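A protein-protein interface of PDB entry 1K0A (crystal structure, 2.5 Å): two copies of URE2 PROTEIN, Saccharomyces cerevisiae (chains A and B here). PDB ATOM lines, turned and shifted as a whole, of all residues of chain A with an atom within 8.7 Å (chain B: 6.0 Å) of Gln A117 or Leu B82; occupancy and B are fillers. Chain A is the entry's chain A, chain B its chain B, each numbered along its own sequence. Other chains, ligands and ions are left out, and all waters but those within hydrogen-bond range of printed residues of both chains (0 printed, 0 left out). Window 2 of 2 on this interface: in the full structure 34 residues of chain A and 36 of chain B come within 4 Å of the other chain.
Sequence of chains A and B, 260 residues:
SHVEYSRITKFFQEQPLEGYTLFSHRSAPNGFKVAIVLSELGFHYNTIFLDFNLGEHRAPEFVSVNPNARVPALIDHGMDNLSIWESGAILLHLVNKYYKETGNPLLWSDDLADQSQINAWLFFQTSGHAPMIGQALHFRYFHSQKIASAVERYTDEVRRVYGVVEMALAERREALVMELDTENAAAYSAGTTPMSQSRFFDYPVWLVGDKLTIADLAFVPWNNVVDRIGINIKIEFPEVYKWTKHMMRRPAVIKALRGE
The backbone carbonyl oxygen of Ser B83 sits at hydrogen-bond distance from the side-chain amide nitrogen of Gln A117, at 2.7 Å.
No position is printed for both chains.
The backbone carbonyl oxygen of Leu B82 sits at hydrogen-bond distance from the backbone NH of Asp B76, 2.6 Å away.
SD of Met B79 sits at hydrogen-bond distance from NE2 of His B93 (3.7 Å).
OG of Ser A116 is in hydrogen-bond range of O of Leu A112 (3.5 Å).
O of Ala A113 sits at hydrogen-bond distance from OG of Ser A116, 2.7 Å away.
N of Met B79 sits at hydrogen-bond distance from OD1 of Asp B76 (3.4 Å).
Of the printed residues of chain B, Leu A112 touches Met B79 (3.6 Å) and His B93 (3.8 Å).
Gln A117 touches just these residues of chain B: Leu B82 (3.8 Å) and Ser B83 (2.7 Å).
Of the printed residues of chain B, Ala A120 touches Trp B85.
Printed residues of chain B within 4 Å of Trp A121: Trp B85.
Of chain A, only Ser A116 and Gln A117 come within 4 Å of Leu B82.
The nearest residue of chain A that does not touch Leu B82 is Ala A113 (4.1 Å).
Of the 12 printed residues of chain B, 5 touch a printed residue of chain A.
Printed residues of chain B that touch a printed residue of chain A: Met B79, Leu B82, Ser B83, Trp B85 and His B93.
Hydrophobic or aromatic side chains of chain B that line the printed part of chain A: Met B79, Leu B82, Trp B85 and His B93.
Of the 24 printed residues of chain A, 6 touch a printed residue of chain B.
Printed residues of chain A that touch a printed residue of chain B: Leu A112, Ser A116, Gln A117, Ala A120, Trp A121 and Phe A124.
Along chain A the printed residues that touch a printed residue of chain B span positions 112 to 124.
Among the printed residues, no Asp or Glu carboxylate lies within 4 Å of a Lys or Arg side-chain nitrogen of the other chain.
Leu A112 touches Met B79.
CD2 of His B93 touches CD1 of Leu A112 (3.8 Å).
OG of Ser A116 touches CD2 of Leu B82 (3.7 Å).
Ser A116 touches His B93 (CB to CD2, 3.5 Å).
NE2 of Gln A117 touches CD1 of Leu B82, 3.8 Å away.
Trp B85 touches Ala A120.
Trp A121 touches Trp B85.
CB of Phe A124 touches CZ3 of Trp B85 (3.6 Å).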
ATOM      1  N   TRP A 108      23.109 -14.213  17.516  1.00  0.00           N
ATOM      2  CA  TRP A 108      22.017 -13.892  18.429  1.00  0.00           C
ATOM      3  C   TRP A 108      21.509 -15.218  18.999  1.00  0.00           C
ATOM      4  O   TRP A 108      22.295 -16.106  19.330  1.00  0.00           O
ATOM      5  CB  TRP A 108      20.919 -13.180  17.623  1.00  0.00           C
ATOM      6  CG  TRP A 108      19.784 -12.503  18.365  1.00  0.00           C
ATOM      7  CD1 TRP A 108      18.491 -12.386  17.929  1.00  0.00           C
ATOM      8  CD2 TRP A 108      19.857 -11.760  19.589  1.00  0.00           C
ATOM      9  NE1 TRP A 108      17.758 -11.615  18.799  1.00  0.00           N
ATOM     10  CE2 TRP A 108      18.567 -11.218  19.826  1.00  0.00           C
ATOM     11  CE3 TRP A 108      20.882 -11.492  20.503  1.00  0.00           C
ATOM     12  CZ2 TRP A 108      18.279 -10.428  20.942  1.00  0.00           C
ATOM     13  CZ3 TRP A 108      20.594 -10.700  21.616  1.00  0.00           C
ATOM     14  CH2 TRP A 108      19.304 -10.178  21.827  1.00  0.00           C
ATOM     15  N   SER A 109      20.194 -15.346  19.097  1.00  0.00           N
ATOM     16  CA  SER A 109      19.563 -16.547  19.615  1.00  0.00           C
ATOM     17  C   SER A 109      18.059 -16.369  19.523  1.00  0.00           C
ATOM     18  O   SER A 109      17.552 -15.255  19.696  1.00  0.00           O
ATOM     19  CB  SER A 109      19.957 -16.770  21.075  1.00  0.00           C
ATOM     20  OG  SER A 109      19.097 -17.715  21.683  1.00  0.00           O
ATOM     21  N   ASP A 111      16.019 -17.976  21.504  1.00  0.00           N
ATOM     22  CA  ASP A 111      15.511 -18.275  22.843  1.00  0.00           C
ATOM     23  C   ASP A 111      15.634 -17.079  23.799  1.00  0.00           C
ATOM     24  O   ASP A 111      16.737 -16.558  24.005  1.00  0.00           O
ATOM     25  CB  ASP A 111      16.269 -19.480  23.400  1.00  0.00           C
ATOM     26  CG  ASP A 111      15.917 -19.772  24.834  1.00  0.00           C
ATOM     27  OD1 ASP A 111      14.705 -19.826  25.152  1.00  0.00           O
ATOM     28  OD2 ASP A 111      16.859 -19.956  25.638  1.00  0.00           O
ATOM     29  N   LEU A 112      14.507 -16.657  24.382  1.00  0.00           N
ATOM     30  CA  LEU A 112      14.473 -15.509  25.298  1.00  0.00           C
ATOM     31  C   LEU A 112      15.561 -15.515  26.370  1.00  0.00           C
ATOM     32  O   LEU A 112      16.220 -14.501  26.596  1.00  0.00           O
ATOM     33  CB  LEU A 112      13.102 -15.392  25.985  1.00  0.00           C
ATOM     34  CG  LEU A 112      13.021 -14.385  27.153  1.00  0.00           C
ATOM     35  CD1 LEU A 112      13.347 -12.966  26.664  1.00  0.00           C
ATOM     36  CD2 LEU A 112      11.628 -14.424  27.792  1.00  0.00           C
ATOM     37  N   ALA A 113      15.744 -16.655  27.027  1.00  0.00           N
ATOM     38  CA  ALA A 113      16.749 -16.768  28.073  1.00  0.00           C
ATOM     39  C   ALA A 113      18.128 -16.334  27.580  1.00  0.00           C
ATOM     40  O   ALA A 113      18.777 -15.495  28.203  1.00  0.00           O
ATOM     41  CB  ALA A 113      16.797 -18.198  28.596  1.00  0.00           C
ATOM     42  N   ASP A 114      18.572 -16.898  26.461  1.00  0.00           N
ATOM     43  CA  ASP A 114      19.879 -16.551  25.911  1.00  0.00           C
ATOM     44  C   ASP A 114      19.954 -15.083  25.512  1.00  0.00           C
ATOM     45  O   ASP A 114      21.004 -14.454  25.640  1.00  0.00           O
ATOM     46  CB  ASP A 114      20.205 -17.427  24.693  1.00  0.00           C
ATOM     47  CG  ASP A 114      20.761 -18.795  25.076  1.00  0.00           C
ATOM     48  OD1 ASP A 114      20.986 -19.628  24.164  1.00  0.00           O
ATOM     49  OD2 ASP A 114      20.984 -19.037  26.285  1.00  0.00           O
ATOM     50  N   GLN A 115      18.840 -14.544  25.023  1.00  0.00           N
ATOM     51  CA  GLN A 115      18.800 -13.146  24.613  1.00  0.00           C
ATOM     52  C   GLN A 115      19.031 -12.200  25.789  1.00  0.00           C
ATOM     53  O   GLN A 115      19.773 -11.220  25.672  1.00  0.00           O
ATOM     54  CB  GLN A 115      17.465 -12.820  23.959  1.00  0.00           C
ATOM     55  CG  GLN A 115      17.208 -13.607  22.703  1.00  0.00           C
ATOM     56  CD  GLN A 115      15.959 -13.151  21.981  1.00  0.00           C
ATOM     57  OE1 GLN A 115      15.490 -13.809  21.051  1.00  0.00           O
ATOM     58  NE2 GLN A 115      15.418 -12.009  22.396  1.00  0.00           N
ATOM     59  N   SER A 116      18.400 -12.497  26.921  1.00  0.00           N
ATOM     60  CA  SER A 116      18.569 -11.662  28.097  1.00  0.00           C
ATOM     61  C   SER A 116      20.024 -11.720  28.589  1.00  0.00           C
ATOM     62  O   SER A 116      20.545 -10.734  29.111  1.00  0.00           O
ATOM     63  CB  SER A 116      17.590 -12.081  29.206  1.00  0.00           C
ATOM     64  OG  SER A 116      17.743 -13.446  29.555  1.00  0.00           O
ATOM     65  N   GLN A 117      20.683 -12.863  28.404  1.00  0.00           N
ATOM     66  CA  GLN A 117      22.078 -12.995  28.817  1.00  0.00           C
ATOM     67  C   GLN A 117      22.942 -12.196  27.854  1.00  0.00           C
ATOM     68  O   GLN A 117      23.898 -11.528  28.265  1.00  0.00           O
ATOM     69  CB  GLN A 117      22.521 -14.464  28.824  1.00  0.00           C
ATOM     70  CG  GLN A 117      21.762 -15.338  29.812  1.00  0.00           C
ATOM     71  CD  GLN A 117      21.810 -14.789  31.220  1.00  0.00           C
ATOM     72  OE1 GLN A 117      22.871 -14.746  31.854  1.00  0.00           O
ATOM     73  NE2 GLN A 117      20.659 -14.350  31.718  1.00  0.00           N
ATOM     74  N   ILE A 118      22.594 -12.254  26.570  1.00  0.00           N
ATOM     75  CA  ILE A 118      23.329 -11.503  25.553  1.00  0.00           C
ATOM     76  C   ILE A 118      23.134 -10.002  25.798  1.00  0.00           C
ATOM     77  O   ILE A 118      24.075  -9.208  25.678  1.00  0.00           O
ATOM     78  CB  ILE A 118      22.848 -11.878  24.131  1.00  0.00           C
ATOM     79  CG1 ILE A 118      23.228 -13.333  23.830  1.00  0.00           C
ATOM     80  CG2 ILE A 118      23.471 -10.951  23.102  1.00  0.00           C
ATOM     81  CD1 ILE A 118      22.568 -13.892  22.593  1.00  0.00           C
ATOM     82  N   ASN A 119      21.919  -9.610  26.170  1.00  0.00           N
ATOM     83  CA  ASN A 119      21.668  -8.199  26.444  1.00  0.00           C
ATOM     84  C   ASN A 119      22.416  -7.748  27.706  1.00  0.00           C
ATOM     85  O   ASN A 119      22.960  -6.648  27.758  1.00  0.00           O
ATOM     86  CB  ASN A 119      20.168  -7.955  26.585  1.00  0.00           C
ATOM     87  CG  ASN A 119      19.428  -8.152  25.279  1.00  0.00           C
ATOM     88  OD1 ASN A 119      18.205  -8.326  25.260  1.00  0.00           O
ATOM     89  ND2 ASN A 119      20.165  -8.130  24.175  1.00  0.00           N
ATOM     90  N   ALA A 120      22.448  -8.615  28.712  1.00  0.00           N
ATOM     91  CA  ALA A 120      23.133  -8.321  29.958  1.00  0.00           C
ATOM     92  C   ALA A 120      24.576  -7.947  29.627  1.00  0.00           C
ATOM     93  O   ALA A 120      25.060  -6.894  30.043  1.00  0.00           O
ATOM     94  CB  ALA A 120      23.082  -9.543  30.887  1.00  0.00           C
ATOM     95  N   TRP A 121      25.247  -8.803  28.855  1.00  0.00           N
ATOM     96  CA  TRP A 121      26.625  -8.537  28.453  1.00  0.00           C
ATOM     97  C   TRP A 121      26.733  -7.277  27.607  1.00  0.00           C
ATOM     98  O   TRP A 121      27.611  -6.442  27.836  1.00  0.00           O
ATOM     99  CB  TRP A 121      27.204  -9.717  27.663  1.00  0.00           C
ATOM    100  CG  TRP A 121      27.593 -10.863  28.532  1.00  0.00           C
ATOM    101  CD1 TRP A 121      26.941 -12.055  28.655  1.00  0.00           C
ATOM    102  CD2 TRP A 121      28.664 -10.892  29.479  1.00  0.00           C
ATOM    103  NE1 TRP A 121      27.531 -12.819  29.629  1.00  0.00           N
ATOM    104  CE2 TRP A 121      28.591 -12.130  30.152  1.00  0.00           C
ATOM    105  CE3 TRP A 121      29.673  -9.989  29.831  1.00  0.00           C
ATOM    106  CZ2 TRP A 121      29.488 -12.488  31.155  1.00  0.00           C
ATOM    107  CZ3 TRP A 121      30.564 -10.344  30.832  1.00  0.00           C
ATOM    108  CH2 TRP A 121      30.464 -11.583  31.484  1.00  0.00           C
ATOM    109  N   LEU A 122      25.839  -7.153  26.630  1.00  0.00           N
ATOM    110  CA  LEU A 122      25.829  -6.009  25.728  1.00  0.00           C
ATOM    111  C   LEU A 122      25.677  -4.683  26.447  1.00  0.00           C
ATOM    112  O   LEU A 122      26.343  -3.711  26.092  1.00  0.00           O
ATOM    113  CB  LEU A 122      24.708  -6.151  24.693  1.00  0.00           C
ATOM    114  CG  LEU A 122      24.517  -4.950  23.754  1.00  0.00           C
ATOM    115  CD1 LEU A 122      25.848  -4.529  23.117  1.00  0.00           C
ATOM    116  CD2 LEU A 122      23.493  -5.323  22.695  1.00  0.00           C
ATOM    117  N   PHE A 123      24.799  -4.632  27.447  1.00  0.00           N
ATOM    118  CA  PHE A 123      24.606  -3.399  28.206  1.00  0.00           C
ATOM    119  C   PHE A 123      25.807  -3.151  29.085  1.00  0.00           C
ATOM    120  O   PHE A 123      26.211  -2.011  29.318  1.00  0.00           O
ATOM    121  CB  PHE A 123      23.363  -3.473  29.101  1.00  0.00           C
ATOM    122  CG  PHE A 123      22.125  -2.977  28.440  1.00  0.00           C
ATOM    123  CD1 PHE A 123      21.208  -3.872  27.875  1.00  0.00           C
ATOM    124  CD2 PHE A 123      21.893  -1.603  28.332  1.00  0.00           C
ATOM    125  CE1 PHE A 123      20.082  -3.406  27.214  1.00  0.00           C
ATOM    126  CE2 PHE A 123      20.770  -1.127  27.668  1.00  0.00           C
ATOM    127  CZ  PHE A 123      19.854  -2.028  27.104  1.00  0.00           C
ATOM    128  N   PHE A 124      26.365  -4.241  29.590  1.00  0.00           N
ATOM    129  CA  PHE A 124      27.515  -4.157  30.451  1.00  0.00           C
ATOM    130  C   PHE A 124      28.699  -3.574  29.676  1.00  0.00           C
ATOM    131  O   PHE A 124      29.441  -2.736  30.196  1.00  0.00           O
ATOM    132  CB  PHE A 124      27.854  -5.538  30.983  1.00  0.00           C
ATOM    133  CG  PHE A 124      29.127  -5.577  31.760  1.00  0.00           C
ATOM    134  CD1 PHE A 124      29.316  -4.731  32.843  1.00  0.00           C
ATOM    135  CD2 PHE A 124      30.138  -6.463  31.418  1.00  0.00           C
ATOM    136  CE1 PHE A 124      30.495  -4.767  33.576  1.00  0.00           C
ATOM    137  CE2 PHE A 124      31.316  -6.506  32.146  1.00  0.00           C
ATOM    138  CZ  PHE A 124      31.494  -5.656  33.228  1.00  0.00           C
ATOM    139  N   ARG A 172      33.592 -20.797  31.551  1.00  0.00           N
ATOM    140  CA  ARG A 172      33.019 -21.396  30.351  1.00  0.00           C
ATOM    141  C   ARG A 172      34.011 -22.440  29.852  1.00  0.00           C
ATOM    142  O   ARG A 172      33.634 -23.434  29.231  1.00  0.00           O
ATOM    143  CB  ARG A 172      32.795 -20.336  29.264  1.00  0.00           C
ATOM    144  CG  ARG A 172      32.023 -19.103  29.709  1.00  0.00           C
ATOM    145  CD  ARG A 172      30.576 -19.397  30.096  1.00  0.00           C
ATOM    146  NE  ARG A 172      29.853 -18.167  30.434  1.00  0.00           N
ATOM    147  CZ  ARG A 172      29.913 -17.547  31.612  1.00  0.00           C
ATOM    148  NH1 ARG A 172      30.657 -18.038  32.596  1.00  0.00           N
ATOM    149  NH2 ARG A 172      29.246 -16.415  31.800  1.00  0.00           N
ATOM    150  N   LEU A 207      30.876 -16.218  25.833  1.00  0.00           N
ATOM    151  CA  LEU A 207      30.040 -15.754  26.923  1.00  0.00           C
ATOM    152  C   LEU A 207      28.663 -16.394  27.011  1.00  0.00           C
ATOM    153  O   LEU A 207      28.239 -16.810  28.088  1.00  0.00           O
ATOM    154  CB  LEU A 207      29.886 -14.237  26.840  1.00  0.00           C
ATOM    155  CG  LEU A 207      31.176 -13.420  26.880  1.00  0.00           C
ATOM    156  CD1 LEU A 207      30.889 -11.955  26.563  1.00  0.00           C
ATOM    157  CD2 LEU A 207      31.811 -13.562  28.248  1.00  0.00           C
ATOM    158  N   VAL A 208      27.965 -16.489  25.887  1.00  0.00           N
ATOM    159  CA  VAL A 208      26.617 -17.050  25.891  1.00  0.00           C
ATOM    160  C   VAL A 208      26.425 -18.166  24.863  1.00  0.00           C
ATOM    161  O   VAL A 208      26.971 -18.110  23.765  1.00  0.00           O
ATOM    162  CB  VAL A 208      25.558 -15.921  25.606  1.00  0.00           C
ATOM    163  CG1 VAL A 208      24.159 -16.455  25.739  1.00  0.00           C
ATOM    164  CG2 VAL A 208      25.758 -14.752  26.548  1.00  0.00           C
ATOM    165  N   GLY A 209      25.640 -19.175  25.236  1.00  0.00           N
ATOM    166  CA  GLY A 209      25.326 -20.290  24.352  1.00  0.00           C
ATOM    167  C   GLY A 209      26.431 -21.048  23.626  1.00  0.00           C
ATOM    168  O   GLY A 209      26.154 -21.727  22.638  1.00  0.00           O
ATOM    169  N   THR A 213      28.471 -14.445  19.657  1.00  0.00           N
ATOM    170  CA  THR A 213      27.337 -13.523  19.585  1.00  0.00           C
ATOM    171  C   THR A 213      27.816 -12.073  19.676  1.00  0.00           C
ATOM    172  O   THR A 213      28.997 -11.803  19.926  1.00  0.00           O
ATOM    173  CB  THR A 213      26.300 -13.748  20.714  1.00  0.00           C
ATOM    174  OG1 THR A 213      26.866 -13.386  21.974  1.00  0.00           O
ATOM    175  CG2 THR A 213      25.846 -15.188  20.747  1.00  0.00           C
ATOM    176  N   ILE A 214      26.898 -11.142  19.464  1.00  0.00           N
ATOM    177  CA  ILE A 214      27.230  -9.734  19.553  1.00  0.00           C
ATOM    178  C   ILE A 214      27.799  -9.443  20.934  1.00  0.00           C
ATOM    179  O   ILE A 214      28.530  -8.471  21.132  1.00  0.00           O
ATOM    180  CB  ILE A 214      25.982  -8.839  19.295  1.00  0.00           C
ATOM    181  CG1 ILE A 214      24.755  -9.398  20.026  1.00  0.00           C
ATOM    182  CG2 ILE A 214      25.717  -8.731  17.803  1.00  0.00           C
ATOM    183  CD1 ILE A 214      23.511  -8.539  19.864  1.00  0.00           C
ATOM    184  N   ALA A 215      27.471 -10.303  21.887  1.00  0.00           N
ATOM    185  CA  ALA A 215      27.959 -10.162  23.257  1.00  0.00           C
ATOM    186  C   ALA A 215      29.483 -10.175  23.264  1.00  0.00           C
ATOM    187  O   ALA A 215      30.117  -9.364  23.932  1.00  0.00           O
ATOM    188  CB  ALA A 215      27.428 -11.298  24.109  1.00  0.00           C
ATOM    189  N   ASP A 216      30.063 -11.102  22.510  1.00  0.00           N
ATOM    190  CA  ASP A 216      31.515 -11.205  22.423  1.00  0.00           C
ATOM    191  C   ASP A 216      32.050 -10.077  21.544  1.00  0.00           C
ATOM    192  O   ASP A 216      32.924  -9.309  21.962  1.00  0.00           O
ATOM    193  CB  ASP A 216      31.926 -12.552  21.812  1.00  0.00           C
ATOM    194  CG  ASP A 216      31.257 -13.731  22.487  1.00  0.00           C
ATOM    195  OD1 ASP A 216      31.578 -14.018  23.660  1.00  0.00           O
ATOM    196  OD2 ASP A 216      30.399 -14.367  21.842  1.00  0.00           O
ATOM    197  N   LEU B  74      18.134  -9.515  38.755  1.00  0.00           N
ATOM    198  CA  LEU B  74      16.790 -10.062  38.875  1.00  0.00           C
ATOM    199  C   LEU B  74      16.731 -11.553  38.590  1.00  0.00           C
ATOM    200  O   LEU B  74      17.302 -12.029  37.610  1.00  0.00           O
ATOM    201  CB  LEU B  74      15.860  -9.347  37.906  1.00  0.00           C
ATOM    202  CG  LEU B  74      14.399  -9.758  38.007  1.00  0.00           C
ATOM    203  CD1 LEU B  74      13.766  -9.000  39.169  1.00  0.00           C
ATOM    204  CD2 LEU B  74      13.677  -9.442  36.704  1.00  0.00           C
ATOM    205  N   ILE B  75      16.032 -12.279  39.456  1.00  0.00           N
ATOM    206  CA  ILE B  75      15.856 -13.717  39.303  1.00  0.00           C
ATOM    207  C   ILE B  75      14.426 -13.932  38.814  1.00  0.00           C
ATOM    208  O   ILE B  75      13.472 -13.475  39.452  1.00  0.00           O
ATOM    209  CB  ILE B  75      16.012 -14.473  40.647  1.00  0.00           C
ATOM    210  CG1 ILE B  75      17.398 -14.229  41.249  1.00  0.00           C
ATOM    211  CG2 ILE B  75      15.751 -15.963  40.437  1.00  0.00           C
ATOM    212  CD1 ILE B  75      18.529 -14.773  40.434  1.00  0.00           C
ATOM    213  N   ASP B  76      14.281 -14.610  37.683  1.00  0.00           N
ATOM    214  CA  ASP B  76      12.965 -14.893  37.114  1.00  0.00           C
ATOM    215  C   ASP B  76      12.600 -16.339  37.471  1.00  0.00           C
ATOM    216  O   ASP B  76      12.911 -17.271  36.719  1.00  0.00           O
ATOM    217  CB  ASP B  76      13.006 -14.738  35.593  1.00  0.00           C
ATOM    218  CG  ASP B  76      11.639 -14.839  34.963  1.00  0.00           C
ATOM    219  OD1 ASP B  76      10.758 -15.497  35.555  1.00  0.00           O
ATOM    220  OD2 ASP B  76      11.448 -14.272  33.867  1.00  0.00           O
ATOM    221  N   HIS B  77      11.948 -16.517  38.617  1.00  0.00           N
ATOM    222  CA  HIS B  77      11.561 -17.839  39.098  1.00  0.00           C
ATOM    223  C   HIS B  77      10.764 -18.671  38.095  1.00  0.00           C
ATOM    224  O   HIS B  77      11.060 -19.847  37.893  1.00  0.00           O
ATOM    225  CB  HIS B  77      10.788 -17.692  40.407  1.00  0.00           C
ATOM    226  CG  HIS B  77      11.547 -16.950  41.461  1.00  0.00           C
ATOM    227  ND1 HIS B  77      12.805 -17.331  41.873  1.00  0.00           N
ATOM    228  CD2 HIS B  77      11.254 -15.817  42.140  1.00  0.00           C
ATOM    229  CE1 HIS B  77      13.258 -16.461  42.757  1.00  0.00           C
ATOM    230  NE2 HIS B  77      12.336 -15.531  42.936  1.00  0.00           N
ATOM    231  N   MET B  79      10.958 -18.854  35.064  1.00  0.00           N
ATOM    232  CA  MET B  79      11.829 -19.398  34.030  1.00  0.00           C
ATOM    233  C   MET B  79      13.021 -20.146  34.627  1.00  0.00           C
ATOM    234  O   MET B  79      14.173 -19.905  34.255  1.00  0.00           O
ATOM    235  CB  MET B  79      12.312 -18.281  33.093  1.00  0.00           C
ATOM    236  CG  MET B  79      11.296 -17.909  32.007  1.00  0.00           C
ATOM    237  SD  MET B  79      11.680 -16.402  31.081  1.00  0.00           S
ATOM    238  CE  MET B  79      12.999 -16.965  30.020  1.00  0.00           C
ATOM    239  N   ASP B  80      12.727 -21.057  35.553  1.00  0.00           N
ATOM    240  CA  ASP B  80      13.749 -21.877  36.213  1.00  0.00           C
ATOM    241  C   ASP B  80      14.829 -21.058  36.893  1.00  0.00           C
ATOM    242  O   ASP B  80      16.022 -21.376  36.807  1.00  0.00           O
ATOM    243  CB  ASP B  80      14.394 -22.836  35.211  1.00  0.00           C
ATOM    244  CG  ASP B  80      13.418 -23.871  34.686  1.00  0.00           C
ATOM    245  OD1 ASP B  80      13.850 -24.714  33.865  1.00  0.00           O
ATOM    246  OD2 ASP B  80      12.229 -23.842  35.094  1.00  0.00           O
ATOM    247  N   ASN B  81      14.396 -20.008  37.580  1.00  0.00           N
ATOM    248  CA  ASN B  81      15.306 -19.128  38.290  1.00  0.00           C
ATOM    249  C   ASN B  81      16.348 -18.525  37.358  1.00  0.00           C
ATOM    250  O   ASN B  81      17.528 -18.447  37.700  1.00  0.00           O
ATOM    251  CB  ASN B  81      15.988 -19.879  39.440  1.00  0.00           C
ATOM    252  CG  ASN B  81      15.005 -20.317  40.517  1.00  0.00           C
ATOM    253  OD1 ASN B  81      14.173 -19.533  40.980  1.00  0.00           O
ATOM    254  ND2 ASN B  81      15.102 -21.572  40.924  1.00  0.00           N
ATOM    255  N   LEU B  82      15.897 -18.113  36.174  1.00  0.00           N
ATOM    256  CA  LEU B  82      16.769 -17.482  35.197  1.00  0.00           C
ATOM    257  C   LEU B  82      17.198 -16.156  35.800  1.00  0.00           C
ATOM    258  O   LEU B  82      16.364 -15.381  36.270  1.00  0.00           O
ATOM    259  CB  LEU B  82      16.030 -17.203  33.888  1.00  0.00           C
ATOM    260  CG  LEU B  82      16.812 -16.247  32.979  1.00  0.00           C
ATOM    261  CD1 LEU B  82      18.017 -16.976  32.370  1.00  0.00           C
ATOM    262  CD2 LEU B  82      15.903 -15.698  31.901  1.00  0.00           C
ATOM    263  N   SER B  83      18.494 -15.887  35.772  1.00  0.00           N
ATOM    264  CA  SER B  83      18.996 -14.645  36.340  1.00  0.00           C
ATOM    265  C   SER B  83      19.347 -13.585  35.281  1.00  0.00           C
ATOM    266  O   SER B  83      20.008 -13.885  34.292  1.00  0.00           O
ATOM    267  CB  SER B  83      20.229 -14.957  37.193  1.00  0.00           C
ATOM    268  OG  SER B  83      20.496 -13.899  38.085  1.00  0.00           O
ATOM    269  N   ILE B  84      18.894 -12.352  35.470  1.00  0.00           N
ATOM    270  CA  ILE B  84      19.242 -11.293  34.525  1.00  0.00           C
ATOM    271  C   ILE B  84      19.970 -10.164  35.265  1.00  0.00           C
ATOM    272  O   ILE B  84      19.590  -9.798  36.376  1.00  0.00           O
ATOM    273  CB  ILE B  84      18.008 -10.669  33.830  1.00  0.00           C
ATOM    274  CG1 ILE B  84      17.132 -11.743  33.169  1.00  0.00           C
ATOM    275  CG2 ILE B  84      18.483  -9.713  32.746  1.00  0.00           C
ATOM    276  CD1 ILE B  84      16.232 -12.498  34.116  1.00  0.00           C
ATOM    277  N   TRP B  85      21.034  -9.630  34.673  1.00  0.00           N
ATOM    278  CA  TRP B  85      21.741  -8.521  35.301  1.00  0.00           C
ATOM    279  C   TRP B  85      21.832  -7.379  34.300  1.00  0.00           C
ATOM    280  O   TRP B  85      21.668  -7.604  33.103  1.00  0.00           O
ATOM    281  CB  TRP B  85      23.121  -8.944  35.795  1.00  0.00           C
ATOM    282  CG  TRP B  85      23.938  -9.711  34.801  1.00  0.00           C
ATOM    283  CD1 TRP B  85      23.713 -10.984  34.354  1.00  0.00           C
ATOM    284  CD2 TRP B  85      25.141  -9.269  34.163  1.00  0.00           C
ATOM    285  NE1 TRP B  85      24.705 -11.359  33.482  1.00  0.00           N
ATOM    286  CE2 TRP B  85      25.593 -10.328  33.345  1.00  0.00           C
ATOM    287  CE3 TRP B  85      25.883  -8.079  34.205  1.00  0.00           C
ATOM    288  CZ2 TRP B  85      26.758 -10.235  32.572  1.00  0.00           C
ATOM    289  CZ3 TRP B  85      27.047  -7.982  33.432  1.00  0.00           C
ATOM    290  CH2 TRP B  85      27.470  -9.056  32.628  1.00  0.00           C
ATOM    291  N   HIS B  93      13.849  -7.606  29.030  1.00  0.00           N
ATOM    292  CA  HIS B  93      13.357  -8.934  29.349  1.00  0.00           C
ATOM    293  C   HIS B  93      11.927  -8.872  29.888  1.00  0.00           C
ATOM    294  O   HIS B  93      11.068  -9.671  29.492  1.00  0.00           O
ATOM    295  CB  HIS B  93      14.279  -9.594  30.375  1.00  0.00           C
ATOM    296  CG  HIS B  93      13.875 -10.986  30.740  1.00  0.00           C
ATOM    297  ND1 HIS B  93      12.947 -11.258  31.722  1.00  0.00           N
ATOM    298  CD2 HIS B  93      14.239 -12.183  30.225  1.00  0.00           C
ATOM    299  CE1 HIS B  93      12.756 -12.563  31.793  1.00  0.00           C
ATOM    300  NE2 HIS B  93      13.528 -13.148  30.895  1.00  0.00           N
